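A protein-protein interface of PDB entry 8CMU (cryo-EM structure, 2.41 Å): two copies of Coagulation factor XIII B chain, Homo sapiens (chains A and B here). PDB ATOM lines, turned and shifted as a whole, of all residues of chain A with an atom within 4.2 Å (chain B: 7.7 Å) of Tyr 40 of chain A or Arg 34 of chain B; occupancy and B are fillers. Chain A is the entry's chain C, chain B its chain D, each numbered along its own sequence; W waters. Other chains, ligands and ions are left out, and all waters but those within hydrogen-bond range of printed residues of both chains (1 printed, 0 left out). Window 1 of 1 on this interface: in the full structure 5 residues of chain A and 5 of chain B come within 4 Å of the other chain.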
ATOM      1  N   PHE A  27      -7.423   3.522   2.862  1.00  0.00           N
ATOM      2  CA  PHE A  27      -7.917   4.166   1.649  1.00  0.00           C
ATOM      3  C   PHE A  27      -9.165   3.460   1.134  1.00  0.00           C
ATOM      4  O   PHE A  27      -9.100   2.264   0.822  1.00  0.00           O
ATOM      5  CB  PHE A  27      -6.829   4.153   0.579  1.00  0.00           C
ATOM      6  CG  PHE A  27      -7.136   5.012  -0.614  1.00  0.00           C
ATOM      7  CD1 PHE A  27      -6.958   6.381  -0.561  1.00  0.00           C
ATOM      8  CD2 PHE A  27      -7.602   4.447  -1.787  1.00  0.00           C
ATOM      9  CE1 PHE A  27      -7.237   7.173  -1.657  1.00  0.00           C
ATOM     10  CE2 PHE A  27      -7.886   5.235  -2.886  1.00  0.00           C
ATOM     11  CZ  PHE A  27      -7.701   6.599  -2.820  1.00  0.00           C
ATOM     12  N   GLY A  33     -17.053   4.269  -8.572  1.00  0.00           N
ATOM     13  CA  GLY A  33     -17.212   5.616  -8.069  1.00  0.00           C
ATOM     14  C   GLY A  33     -15.888   6.197  -7.624  1.00  0.00           C
ATOM     15  O   GLY A  33     -14.828   5.602  -7.831  1.00  0.00           O
ATOM     16  N   ARG A  34     -15.955   7.377  -7.003  1.00  0.00           N
ATOM     17  CA  ARG A  34     -14.733   8.085  -6.649  1.00  0.00           C
ATOM     18  C   ARG A  34     -14.892   8.809  -5.318  1.00  0.00           C
ATOM     19  O   ARG A  34     -15.999   9.159  -4.900  1.00  0.00           O
ATOM     20  CB  ARG A  34     -14.387   9.156  -7.697  1.00  0.00           C
ATOM     21  CG  ARG A  34     -14.195   8.711  -9.143  1.00  0.00           C
ATOM     22  CD  ARG A  34     -12.904   7.977  -9.424  1.00  0.00           C
ATOM     23  NE  ARG A  34     -13.170   6.677 -10.026  1.00  0.00           N
ATOM     24  CZ  ARG A  34     -12.939   6.384 -11.300  1.00  0.00           C
ATOM     25  NH1 ARG A  34     -12.429   7.277 -12.132  1.00  0.00           N
ATOM     26  NH2 ARG A  34     -13.234   5.168 -11.751  1.00  0.00           N
ATOM     27  N   ILE A  35     -13.754   9.037  -4.658  1.00  0.00           N
ATOM     28  CA  ILE A  35     -13.605  10.044  -3.608  1.00  0.00           C
ATOM     29  C   ILE A  35     -13.055  11.324  -4.229  1.00  0.00           C
ATOM     30  O   ILE A  35     -12.756  11.360  -5.428  1.00  0.00           O
ATOM     31  CB  ILE A  35     -12.724   9.542  -2.448  1.00  0.00           C
ATOM     32  CG1 ILE A  35     -11.284   9.312  -2.906  1.00  0.00           C
ATOM     33  CG2 ILE A  35     -13.325   8.311  -1.804  1.00  0.00           C
ATOM     34  CD1 ILE A  35     -10.395   8.786  -1.810  1.00  0.00           C
ATOM     35  N   GLN A  37     -10.724  13.842  -5.697  1.00  0.00           N
ATOM     36  CA  GLN A  37      -9.694  13.260  -6.551  1.00  0.00           C
ATOM     37  C   GLN A  37      -8.268  13.658  -6.179  1.00  0.00           C
ATOM     38  O   GLN A  37      -7.332  13.049  -6.707  1.00  0.00           O
ATOM     39  CB  GLN A  37      -9.950  13.636  -8.010  1.00  0.00           C
ATOM     40  CG  GLN A  37      -9.664  15.089  -8.337  1.00  0.00           C
ATOM     41  CD  GLN A  37      -9.984  15.434  -9.776  1.00  0.00           C
ATOM     42  OE1 GLN A  37      -9.716  16.544 -10.234  1.00  0.00           O
ATOM     43  NE2 GLN A  37     -10.557  14.481 -10.500  1.00  0.00           N
ATOM     44  N   TYR A  38      -8.062  14.643  -5.299  1.00  0.00           N
ATOM     45  CA  TYR A  38      -6.714  14.856  -4.771  1.00  0.00           C
ATOM     46  C   TYR A  38      -6.257  13.719  -3.867  1.00  0.00           C
ATOM     47  O   TYR A  38      -5.053  13.462  -3.767  1.00  0.00           O
ATOM     48  CB  TYR A  38      -6.604  16.198  -4.039  1.00  0.00           C
ATOM     49  CG  TYR A  38      -7.733  16.556  -3.100  1.00  0.00           C
ATOM     50  CD1 TYR A  38      -7.737  16.109  -1.786  1.00  0.00           C
ATOM     51  CD2 TYR A  38      -8.759  17.395  -3.508  1.00  0.00           C
ATOM     52  CE1 TYR A  38      -8.764  16.430  -0.928  1.00  0.00           C
ATOM     53  CE2 TYR A  38      -9.780  17.742  -2.650  1.00  0.00           C
ATOM     54  CZ  TYR A  38      -9.781  17.252  -1.362  1.00  0.00           C
ATOM     55  OH  TYR A  38     -10.787  17.613  -0.497  1.00  0.00           O
ATOM     56  N   TYR A  39      -7.189  13.037  -3.196  1.00  0.00           N
ATOM     57  CA  TYR A  39      -6.812  11.941  -2.309  1.00  0.00           C
ATOM     58  C   TYR A  39      -6.078  10.827  -3.047  1.00  0.00           C
ATOM     59  O   TYR A  39      -5.279  10.107  -2.440  1.00  0.00           O
ATOM     60  CB  TYR A  39      -8.048  11.375  -1.613  1.00  0.00           C
ATOM     61  CG  TYR A  39      -8.665  12.289  -0.581  1.00  0.00           C
ATOM     62  CD1 TYR A  39      -9.989  12.685  -0.682  1.00  0.00           C
ATOM     63  CD2 TYR A  39      -7.923  12.752   0.498  1.00  0.00           C
ATOM     64  CE1 TYR A  39     -10.561  13.513   0.260  1.00  0.00           C
ATOM     65  CE2 TYR A  39      -8.486  13.585   1.443  1.00  0.00           C
ATOM     66  CZ  TYR A  39      -9.806  13.961   1.319  1.00  0.00           C
ATOM     67  OH  TYR A  39     -10.371  14.795   2.254  1.00  0.00           O
ATOM     68  N   TYR A  40      -6.344  10.654  -4.344  1.00  0.00           N
ATOM     69  CA  TYR A  40      -5.586   9.688  -5.133  1.00  0.00           C
ATOM     70  C   TYR A  40      -4.125  10.089  -5.306  1.00  0.00           C
ATOM     71  O   TYR A  40      -3.249   9.219  -5.337  1.00  0.00           O
ATOM     72  CB  TYR A  40      -6.248   9.500  -6.497  1.00  0.00           C
ATOM     73  CG  TYR A  40      -7.626   8.893  -6.409  1.00  0.00           C
ATOM     74  CD1 TYR A  40      -7.795   7.520  -6.304  1.00  0.00           C
ATOM     75  CD2 TYR A  40      -8.758   9.695  -6.404  1.00  0.00           C
ATOM     76  CE1 TYR A  40      -9.053   6.959  -6.241  1.00  0.00           C
ATOM     77  CE2 TYR A  40     -10.020   9.146  -6.316  1.00  0.00           C
ATOM     78  CZ  TYR A  40     -10.163   7.778  -6.241  1.00  0.00           C
ATOM     79  OH  TYR A  40     -11.420   7.232  -6.126  1.00  0.00           O
ATOM     80  N   THR A  41      -3.839  11.387  -5.412  1.00  0.00           N
ATOM     81  CA  THR A  41      -2.453  11.830  -5.535  1.00  0.00           C
ATOM     82  C   THR A  41      -1.763  11.883  -4.177  1.00  0.00           C
ATOM     83  O   THR A  41      -0.638  11.394  -4.022  1.00  0.00           O
ATOM     84  CB  THR A  41      -2.396  13.196  -6.222  1.00  0.00           C
ATOM     85  OG1 THR A  41      -2.887  13.079  -7.562  1.00  0.00           O
ATOM     86  CG2 THR A  41      -0.971  13.718  -6.262  1.00  0.00           C
ATOM     87  N   PHE A  42      -2.425  12.475  -3.185  1.00  0.00           N
ATOM     88  CA  PHE A  42      -1.864  12.697  -1.858  1.00  0.00           C
ATOM     89  C   PHE A  42      -2.192  11.565  -0.892  1.00  0.00           C
ATOM     90  O   PHE A  42      -2.321  11.795   0.318  1.00  0.00           O
ATOM     91  CB  PHE A  42      -2.331  14.048  -1.320  1.00  0.00           C
ATOM     92  CG  PHE A  42      -1.806  15.211  -2.114  1.00  0.00           C
ATOM     93  CD1 PHE A  42      -2.467  15.640  -3.253  1.00  0.00           C
ATOM     94  CD2 PHE A  42      -0.627  15.837  -1.758  1.00  0.00           C
ATOM     95  CE1 PHE A  42      -1.982  16.696  -3.999  1.00  0.00           C
ATOM     96  CE2 PHE A  42      -0.134  16.890  -2.503  1.00  0.00           C
ATOM     97  CZ  PHE A  42      -0.814  17.322  -3.624  1.00  0.00           C
ATOM     98  N   LYS A  43      -2.352  10.349  -1.420  1.00  0.00           N
ATOM     99  CA  LYS A  43      -2.817   9.198  -0.652  1.00  0.00           C
ATOM    100  C   LYS A  43      -1.975   8.950   0.597  1.00  0.00           C
ATOM    101  O   LYS A  43      -2.511   8.765   1.695  1.00  0.00           O
ATOM    102  CB  LYS A  43      -2.803   7.966  -1.561  1.00  0.00           C
ATOM    103  CG  LYS A  43      -3.387   6.703  -0.975  1.00  0.00           C
ATOM    104  CD  LYS A  43      -3.273   5.564  -1.981  1.00  0.00           C
ATOM    105  CE  LYS A  43      -3.960   5.918  -3.291  1.00  0.00           C
ATOM    106  NZ  LYS A  43      -4.330   4.712  -4.082  1.00  0.00           N
ATOM    107  N   PRO B  28      -8.006  -0.649 -20.523  1.00  0.00           N
ATOM    108  CA  PRO B  28      -6.701  -0.736 -19.859  1.00  0.00           C
ATOM    109  C   PRO B  28      -6.812  -0.434 -18.373  1.00  0.00           C
ATOM    110  O   PRO B  28      -7.569   0.443 -17.952  1.00  0.00           O
ATOM    111  CB  PRO B  28      -5.864   0.321 -20.589  1.00  0.00           C
ATOM    112  CG  PRO B  28      -6.864   1.331 -21.028  1.00  0.00           C
ATOM    113  CD  PRO B  28      -8.108   0.546 -21.376  1.00  0.00           C
ATOM    114  N   HIS B  29      -6.042  -1.174 -17.574  1.00  0.00           N
ATOM    115  CA  HIS B  29      -5.958  -0.932 -16.134  1.00  0.00           C
ATOM    116  C   HIS B  29      -4.700  -0.127 -15.821  1.00  0.00           C
ATOM    117  O   HIS B  29      -3.652  -0.668 -15.471  1.00  0.00           O
ATOM    118  CB  HIS B  29      -5.986  -2.253 -15.369  1.00  0.00           C
ATOM    119  CG  HIS B  29      -6.352  -2.106 -13.925  1.00  0.00           C
ATOM    120  ND1 HIS B  29      -5.598  -1.367 -13.040  1.00  0.00           N
ATOM    121  CD2 HIS B  29      -7.395  -2.597 -13.214  1.00  0.00           C
ATOM    122  CE1 HIS B  29      -6.157  -1.413 -11.844  1.00  0.00           C
ATOM    123  NE2 HIS B  29      -7.249  -2.152 -11.922  1.00  0.00           N
ATOM    124  N   VAL B  30      -4.812   1.193 -15.952  1.00  0.00           N
ATOM    125  CA  VAL B  30      -3.653   2.061 -15.771  1.00  0.00           C
ATOM    126  C   VAL B  30      -3.454   2.253 -14.274  1.00  0.00           C
ATOM    127  O   VAL B  30      -4.073   3.128 -13.659  1.00  0.00           O
ATOM    128  CB  VAL B  30      -3.827   3.406 -16.498  1.00  0.00           C
ATOM    129  CG1 VAL B  30      -2.501   4.148 -16.563  1.00  0.00           C
ATOM    130  CG2 VAL B  30      -4.383   3.184 -17.894  1.00  0.00           C
ATOM    131  N   GLU B  31      -2.594   1.431 -13.682  1.00  0.00           N
ATOM    132  CA  GLU B  31      -2.233   1.583 -12.279  1.00  0.00           C
ATOM    133  C   GLU B  31      -1.417   2.850 -12.052  1.00  0.00           C
ATOM    134  O   GLU B  31      -0.491   3.149 -12.814  1.00  0.00           O
ATOM    135  CB  GLU B  31      -1.450   0.360 -11.803  1.00  0.00           C
ATOM    136  CG  GLU B  31      -1.062   0.370 -10.325  1.00  0.00           C
ATOM    137  CD  GLU B  31      -2.229   0.111  -9.380  1.00  0.00           C
ATOM    138  OE1 GLU B  31      -1.978  -0.370  -8.256  1.00  0.00           O
ATOM    139  OE2 GLU B  31      -3.394   0.378  -9.748  1.00  0.00           O
ATOM    140  N   ASN B  32      -1.765   3.594 -11.000  1.00  0.00           N
ATOM    141  CA  ASN B  32      -1.178   4.899 -10.693  1.00  0.00           C
ATOM    142  C   ASN B  32      -1.371   5.930 -11.804  1.00  0.00           C
ATOM    143  O   ASN B  32      -0.647   6.929 -11.853  1.00  0.00           O
ATOM    144  CB  ASN B  32       0.308   4.763 -10.349  1.00  0.00           C
ATOM    145  CG  ASN B  32       0.579   3.613  -9.397  1.00  0.00           C
ATOM    146  OD1 ASN B  32      -0.004   3.535  -8.317  1.00  0.00           O
ATOM    147  ND2 ASN B  32       1.463   2.707  -9.800  1.00  0.00           N
ATOM    148  N   GLY B  33      -2.326   5.715 -12.704  1.00  0.00           N
ATOM    149  CA  GLY B  33      -2.505   6.609 -13.833  1.00  0.00           C
ATOM    150  C   GLY B  33      -3.935   6.618 -14.332  1.00  0.00           C
ATOM    151  O   GLY B  33      -4.814   6.040 -13.686  1.00  0.00           O
ATOM    152  N   ARG B  34      -4.193   7.260 -15.471  1.00  0.00           N
ATOM    153  CA  ARG B  34      -5.562   7.417 -15.936  1.00  0.00           C
ATOM    154  C   ARG B  34      -5.576   7.456 -17.457  1.00  0.00           C
ATOM    155  O   ARG B  34      -4.616   7.911 -18.090  1.00  0.00           O
ATOM    156  CB  ARG B  34      -6.179   8.730 -15.426  1.00  0.00           C
ATOM    157  CG  ARG B  34      -6.268   8.919 -13.913  1.00  0.00           C
ATOM    158  CD  ARG B  34      -7.460   8.265 -13.252  1.00  0.00           C
ATOM    159  NE  ARG B  34      -7.026   7.432 -12.137  1.00  0.00           N
ATOM    160  CZ  ARG B  34      -7.256   7.713 -10.860  1.00  0.00           C
ATOM    161  NH1 ARG B  34      -7.920   8.800 -10.500  1.00  0.00           N
ATOM    162  NH2 ARG B  34      -6.796   6.892  -9.922  1.00  0.00           N
ATOM    163  N   ILE B  35      -6.681   6.975 -18.039  1.00  0.00           N
ATOM    164  CA  ILE B  35      -7.110   7.360 -19.382  1.00  0.00           C
ATOM    165  C   ILE B  35      -8.153   8.470 -19.291  1.00  0.00           C
ATOM    166  O   ILE B  35      -8.546   8.873 -18.190  1.00  0.00           O
ATOM    167  CB  ILE B  35      -7.633   6.153 -20.179  1.00  0.00           C
ATOM    168  CG1 ILE B  35      -8.816   5.497 -19.470  1.00  0.00           C
ATOM    169  CG2 ILE B  35      -6.518   5.146 -20.408  1.00  0.00           C
ATOM    170  CD1 ILE B  35      -9.444   4.399 -20.280  1.00  0.00           C
ATOM    171  N   ALA B  36      -8.587   8.984 -20.445  1.00  0.00           N
ATOM    172  CA  ALA B  36      -9.584  10.050 -20.490  1.00  0.00           C
ATOM    173  C   ALA B  36     -10.840   9.689 -19.699  1.00  0.00           C
ATOM    174  O   ALA B  36     -11.354   8.571 -19.791  1.00  0.00           O
ATOM    175  CB  ALA B  36      -9.953  10.365 -21.941  1.00  0.00           C
ATOM    176  N   GLN B  37     -11.321  10.654 -18.909  1.00  0.00           N
ATOM    177  CA  GLN B  37     -12.263  10.356 -17.834  1.00  0.00           C
ATOM    178  C   GLN B  37     -13.589   9.780 -18.328  1.00  0.00           C
ATOM    179  O   GLN B  37     -14.152   8.889 -17.677  1.00  0.00           O
ATOM    180  CB  GLN B  37     -12.540  11.624 -17.025  1.00  0.00           C
ATOM    181  CG  GLN B  37     -11.705  11.783 -15.768  1.00  0.00           C
ATOM    182  CD  GLN B  37     -11.687  13.215 -15.269  1.00  0.00           C
ATOM    183  OE1 GLN B  37     -10.719  13.656 -14.651  1.00  0.00           O
ATOM    184  NE2 GLN B  37     -12.754  13.955 -15.553  1.00  0.00           N
ATOM    185  N   TYR B  40     -14.122   5.994 -18.385  1.00  0.00           N
ATOM    186  CA  TYR B  40     -14.563   5.329 -17.163  1.00  0.00           C
ATOM    187  C   TYR B  40     -16.081   5.206 -17.082  1.00  0.00           C
ATOM    188  O   TYR B  40     -16.591   4.207 -16.562  1.00  0.00           O
ATOM    189  CB  TYR B  40     -14.000   6.063 -15.948  1.00  0.00           C
ATOM    190  CG  TYR B  40     -12.499   5.918 -15.856  1.00  0.00           C
ATOM    191  CD1 TYR B  40     -11.924   4.809 -15.251  1.00  0.00           C
ATOM    192  CD2 TYR B  40     -11.657   6.870 -16.413  1.00  0.00           C
ATOM    193  CE1 TYR B  40     -10.555   4.689 -15.144  1.00  0.00           C
ATOM    194  CE2 TYR B  40     -10.286   6.738 -16.343  1.00  0.00           C
ATOM    195  CZ  TYR B  40      -9.739   5.651 -15.698  1.00  0.00           C
ATOM    196  OH  TYR B  40      -8.375   5.500 -15.663  1.00  0.00           O
ATOM    197  N   LEU B  55      -4.774   5.528 -27.776  1.00  0.00           N
ATOM    198  CA  LEU B  55      -5.384   5.950 -26.519  1.00  0.00           C
ATOM    199  C   LEU B  55      -4.324   6.609 -25.648  1.00  0.00           C
ATOM    200  O   LEU B  55      -3.349   5.962 -25.250  1.00  0.00           O
ATOM    201  CB  LEU B  55      -6.007   4.750 -25.806  1.00  0.00           C
ATOM    202  CG  LEU B  55      -6.691   4.968 -24.462  1.00  0.00           C
ATOM    203  CD1 LEU B  55      -7.860   5.914 -24.623  1.00  0.00           C
ATOM    204  CD2 LEU B  55      -7.147   3.638 -23.892  1.00  0.00           C
ATOM    205  N   SER B  56      -4.484   7.906 -25.397  1.00  0.00           N
ATOM    206  CA  SER B  56      -3.586   8.619 -24.497  1.00  0.00           C
ATOM    207  C   SER B  56      -3.854   8.246 -23.043  1.00  0.00           C
ATOM    208  O   SER B  56      -5.003   8.049 -22.635  1.00  0.00           O
ATOM    209  CB  SER B  56      -3.729  10.127 -24.687  1.00  0.00           C
ATOM    210  OG  SER B  56      -3.432  10.498 -26.020  1.00  0.00           O
ATOM    211  N   PHE B  57      -2.782   8.151 -22.261  1.00  0.00           N
ATOM    212  CA  PHE B  57      -2.858   7.961 -20.821  1.00  0.00           C
ATOM    213  C   PHE B  57      -1.815   8.847 -20.151  1.00  0.00           C
ATOM    214  O   PHE B  57      -0.873   9.326 -20.791  1.00  0.00           O
ATOM    215  CB  PHE B  57      -2.675   6.486 -20.427  1.00  0.00           C
ATOM    216  CG  PHE B  57      -1.245   6.020 -20.427  1.00  0.00           C
ATOM    217  CD1 PHE B  57      -0.622   5.660 -21.609  1.00  0.00           C
ATOM    218  CD2 PHE B  57      -0.530   5.928 -19.245  1.00  0.00           C
ATOM    219  CE1 PHE B  57       0.689   5.225 -21.613  1.00  0.00           C
ATOM    220  CE2 PHE B  57       0.781   5.496 -19.244  1.00  0.00           C
ATOM    221  CZ  PHE B  57       1.391   5.144 -20.429  1.00  0.00           C
ATOM    222  N   PHE B  58      -1.996   9.074 -18.850  1.00  0.00           N
ATOM    223  CA  PHE B  58      -1.039   9.890 -18.111  1.00  0.00           C
ATOM    224  C   PHE B  58      -0.917   9.361 -16.691  1.00  0.00           C
ATOM    225  O   PHE B  58      -1.869   8.813 -16.132  1.00  0.00           O
ATOM    226  CB  PHE B  58      -1.420  11.378 -18.052  1.00  0.00           C
ATOM    227  CG  PHE B  58      -2.657  11.666 -17.248  1.00  0.00           C
ATOM    228  CD1 PHE B  58      -3.913  11.505 -17.792  1.00  0.00           C
ATOM    229  CD2 PHE B  58      -2.555  12.101 -15.935  1.00  0.00           C
ATOM    230  CE1 PHE B  58      -5.048  11.768 -17.049  1.00  0.00           C
ATOM    231  CE2 PHE B  58      -3.684  12.365 -15.185  1.00  0.00           C
ATOM    232  CZ  PHE B  58      -4.933  12.199 -15.744  1.00  0.00           C
ATOM    233  N   CYS B  59       0.257   9.559 -16.103  1.00  0.00           N
ATOM    234  CA  CYS B  59       0.497   9.168 -14.723  1.00  0.00           C
ATOM    235  C   CYS B  59       0.145  10.295 -13.761  1.00  0.00           C
ATOM    236  O   CYS B  59       0.232  11.478 -14.098  1.00  0.00           O
ATOM    237  CB  CYS B  59       1.961   8.775 -14.539  1.00  0.00           C
ATOM    238  SG  CYS B  59       2.513   7.481 -15.659  1.00  0.00           S
ATOM    239  N   LEU B  60      -0.262   9.909 -12.554  1.00  0.00           N
ATOM    240  CA  LEU B  60      -0.421  10.859 -11.464  1.00  0.00           C
ATOM    241  C   LEU B  60       0.921  11.486 -11.092  1.00  0.00           C
ATOM    242  O   LEU B  60       1.993  10.994 -11.455  1.00  0.00           O
ATOM    243  CB  LEU B  60      -1.037  10.179 -10.241  1.00  0.00           C
ATOM    244  CG  LEU B  60      -2.436   9.579 -10.407  1.00  0.00           C
ATOM    245  CD1 LEU B  60      -2.878   8.884  -9.129  1.00  0.00           C
ATOM    246  CD2 LEU B  60      -3.436  10.649 -10.807  1.00  0.00           C
ATOM    247  N   ALA B  61       0.848  12.596 -10.361  1.00  0.00           N
ATOM    248  CA  ALA B  61       2.034  13.163  -9.738  1.00  0.00           C
ATOM    249  C   ALA B  61       2.715  12.126  -8.850  1.00  0.00           C
ATOM    250  O   ALA B  61       2.063  11.302  -8.205  1.00  0.00           O
ATOM    251  CB  ALA B  61       1.668  14.401  -8.921  1.00  0.00           C
ATOM    252  N   TYR B  63       4.531   9.839 -10.204  1.00  0.00           N
ATOM    253  CA  TYR B  63       4.712   8.694 -11.081  1.00  0.00           C
ATOM    254  C   TYR B  63       5.046   9.188 -12.480  1.00  0.00           C
ATOM    255  O   TYR B  63       4.786  10.340 -12.833  1.00  0.00           O
ATOM    256  CB  TYR B  63       3.459   7.808 -11.122  1.00  0.00           C
ATOM    257  CG  TYR B  63       3.103   7.189  -9.790  1.00  0.00           C
ATOM    258  CD1 TYR B  63       2.368   7.894  -8.847  1.00  0.00           C
ATOM    259  CD2 TYR B  63       3.502   5.899  -9.474  1.00  0.00           C
ATOM    260  CE1 TYR B  63       2.040   7.335  -7.629  1.00  0.00           C
ATOM    261  CE2 TYR B  63       3.183   5.330  -8.257  1.00  0.00           C
ATOM    262  CZ  TYR B  63       2.450   6.052  -7.339  1.00  0.00           C
ATOM    263  OH  TYR B  63       2.129   5.491  -6.125  1.00  0.00           O
ATOM    264  N   GLN B  70       5.129  12.445 -18.723  1.00  0.00           N
ATOM    265  CA  GLN B  70       3.879  12.421 -17.973  1.00  0.00           C
ATOM    266  C   GLN B  70       2.696  11.878 -18.766  1.00  0.00           C
ATOM    267  O   GLN B  70       1.829  11.217 -18.184  1.00  0.00           O
ATOM    268  CB  GLN B  70       3.546  13.827 -17.469  1.00  0.00           C
ATOM    269  CG  GLN B  70       2.647  13.851 -16.245  1.00  0.00           C
ATOM    270  CD  GLN B  70       3.323  13.274 -15.016  1.00  0.00           C
ATOM    271  OE1 GLN B  70       4.487  13.564 -14.740  1.00  0.00           O
ATOM    272  NE2 GLN B  70       2.593  12.455 -14.270  1.00  0.00           N
ATOM    273  N   GLU B  71       2.637  12.130 -20.071  1.00  0.00           N
ATOM    274  CA  GLU B  71       1.539  11.681 -20.919  1.00  0.00           C
ATOM    275  C   GLU B  71       2.078  10.967 -22.149  1.00  0.00           C
ATOM    276  O   GLU B  71       3.048  11.419 -22.761  1.00  0.00           O
ATOM    277  CB  GLU B  71       0.645  12.851 -21.343  1.00  0.00           C
ATOM    278  CG  GLU B  71      -0.520  12.445 -22.230  1.00  0.00           C
ATOM    279  CD  GLU B  71      -1.092  13.608 -23.013  1.00  0.00           C
ATOM    280  OE1 GLU B  71      -1.043  14.748 -22.506  1.00  0.00           O
ATOM    281  OE2 GLU B  71      -1.590  13.384 -24.135  1.00  0.00           O
ATOM    282  N   GLU B  72       1.454   9.846 -22.507  1.00  0.00           N
ATOM    283  CA  GLU B  72       1.941   9.042 -23.620  1.00  0.00           C
ATOM    284  C   GLU B  72       0.761   8.308 -24.248  1.00  0.00           C
ATOM    285  O   GLU B  72      -0.271   8.098 -23.611  1.00  0.00           O
ATOM    286  CB  GLU B  72       3.055   8.092 -23.139  1.00  0.00           C
ATOM    287  CG  GLU B  72       3.088   6.697 -23.743  1.00  0.00           C
ATOM    288  CD  GLU B  72       3.940   5.738 -22.935  1.00  0.00           C
ATOM    289  OE1 GLU B  72       3.706   4.516 -23.019  1.00  0.00           O
ATOM    290  OE2 GLU B  72       4.851   6.209 -22.222  1.00  0.00           O
ATOM    291  N   PRO B  85       0.570   0.223 -20.617  1.00  0.00           N
ATOM    292  CA  PRO B  85       0.229   1.330 -19.713  1.00  0.00           C
ATOM    293  C   PRO B  85       0.605   1.049 -18.267  1.00  0.00           C
ATOM    294  O   PRO B  85      -0.250   0.676 -17.458  1.00  0.00           O
ATOM    295  CB  PRO B  85      -1.295   1.452 -19.871  1.00  0.00           C
ATOM    296  CG  PRO B  85      -1.584   0.851 -21.205  1.00  0.00           C
ATOM    297  CD  PRO B  85      -0.626  -0.306 -21.289  1.00  0.00           C
ATOM    298  N   CYS B  87       2.757   2.929 -14.914  1.00  0.00           N
ATOM    299  CA  CYS B  87       3.317   4.140 -14.328  1.00  0.00           C
ATOM    300  C   CYS B  87       4.201   3.764 -13.150  1.00  0.00           C
ATOM    301  O   CYS B  87       3.743   3.098 -12.216  1.00  0.00           O
ATOM    302  CB  CYS B  87       2.207   5.091 -13.874  1.00  0.00           C
ATOM    303  SG  CYS B  87       1.327   5.899 -15.214  1.00  0.00           S
HETATM  304  O   HOH W   1     -10.813  11.526 -12.162  1.00  0.00           O
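Arg 34 of chain A touches Tyr 40 of chain B, and with the chains exchanged Tyr 40 of chain A touches Arg 34 of chain B.
Among the printed residues, pairs that only touch across the chains: Arg 34 of chain A with Tyr 40 of chain B (3.8 Å), Tyr 40 of chain A with Arg 34 of chain B (3.8 Å), Tyr 40 of chain A with Leu 60 of chain B (3.8 Å) and Thr 41 of chain A with Ala 61 of chain B (3.8 Å).
Water W1 lies within hydrogen-bond range of the side-chain amide oxygen of Gln 37 of chain B (3.3 Å) and the side-chain amide nitrogen of Gln 37 of chain A (3.4 Å).
Of the printed residues of chain B, Arg 34 of chain A touches Tyr 40. Tyr 40 of chain A touches two residues of chain B. Printed residues of chain B within 4 Å of Thr 41 of chain A: Ala 61. Glu 31 of chain B touches none of the printed residues of chain A. Printed residues of chain A within 4 Å of Tyr 40 of chain B: Arg 34 (3.8 Å). The nearest residue of chain B that does not touch Tyr 40 of chain A is Tyr 63 of chain B (6.1 Å). The nearest printed residue of chain A that does not touch Arg 34 of chain B is Arg 34 of chain A (5.0 Å).
Hydrophobic or aromatic side chains of chain B within 4 Å of the printed part of chain A: Tyr 40, Leu 60 and Ala 61. Among the printed residues, 4 pairs touch across the chains. Among the printed residues, no Asp or Glu carboxylate lies within 4 Å of a Lys or Arg side-chain nitrogen of the other chain.
OH of Tyr 40 of chain A is in hydrogen-bond range of N of Ile 35 of chain A (3.3 Å). The backbone carbonyl oxygen (O) of Asn 32 of chain B lies within hydrogen-bond range of the backbone NH (N) of Leu 60 of chain B (3.1 Å). The backbone carbonyl oxygen of Leu 60 of chain B sits at hydrogen-bond distance from the side-chain amide nitrogen of Gln 70 of chain B (3.2 Å). SG of Cys 59 of chain B is disulfide-bonded to SG of Cys 87 of chain B (2.0 Å). The side-chain hydroxyl of Tyr 40 of chain B lies within hydrogen-bond range of the backbone NH of Ile 35 of chain B (3.3 Å). O of Phe 58 of chain B lies within hydrogen-bond range of N of Arg 34 of chain B, 2.9 Å away.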
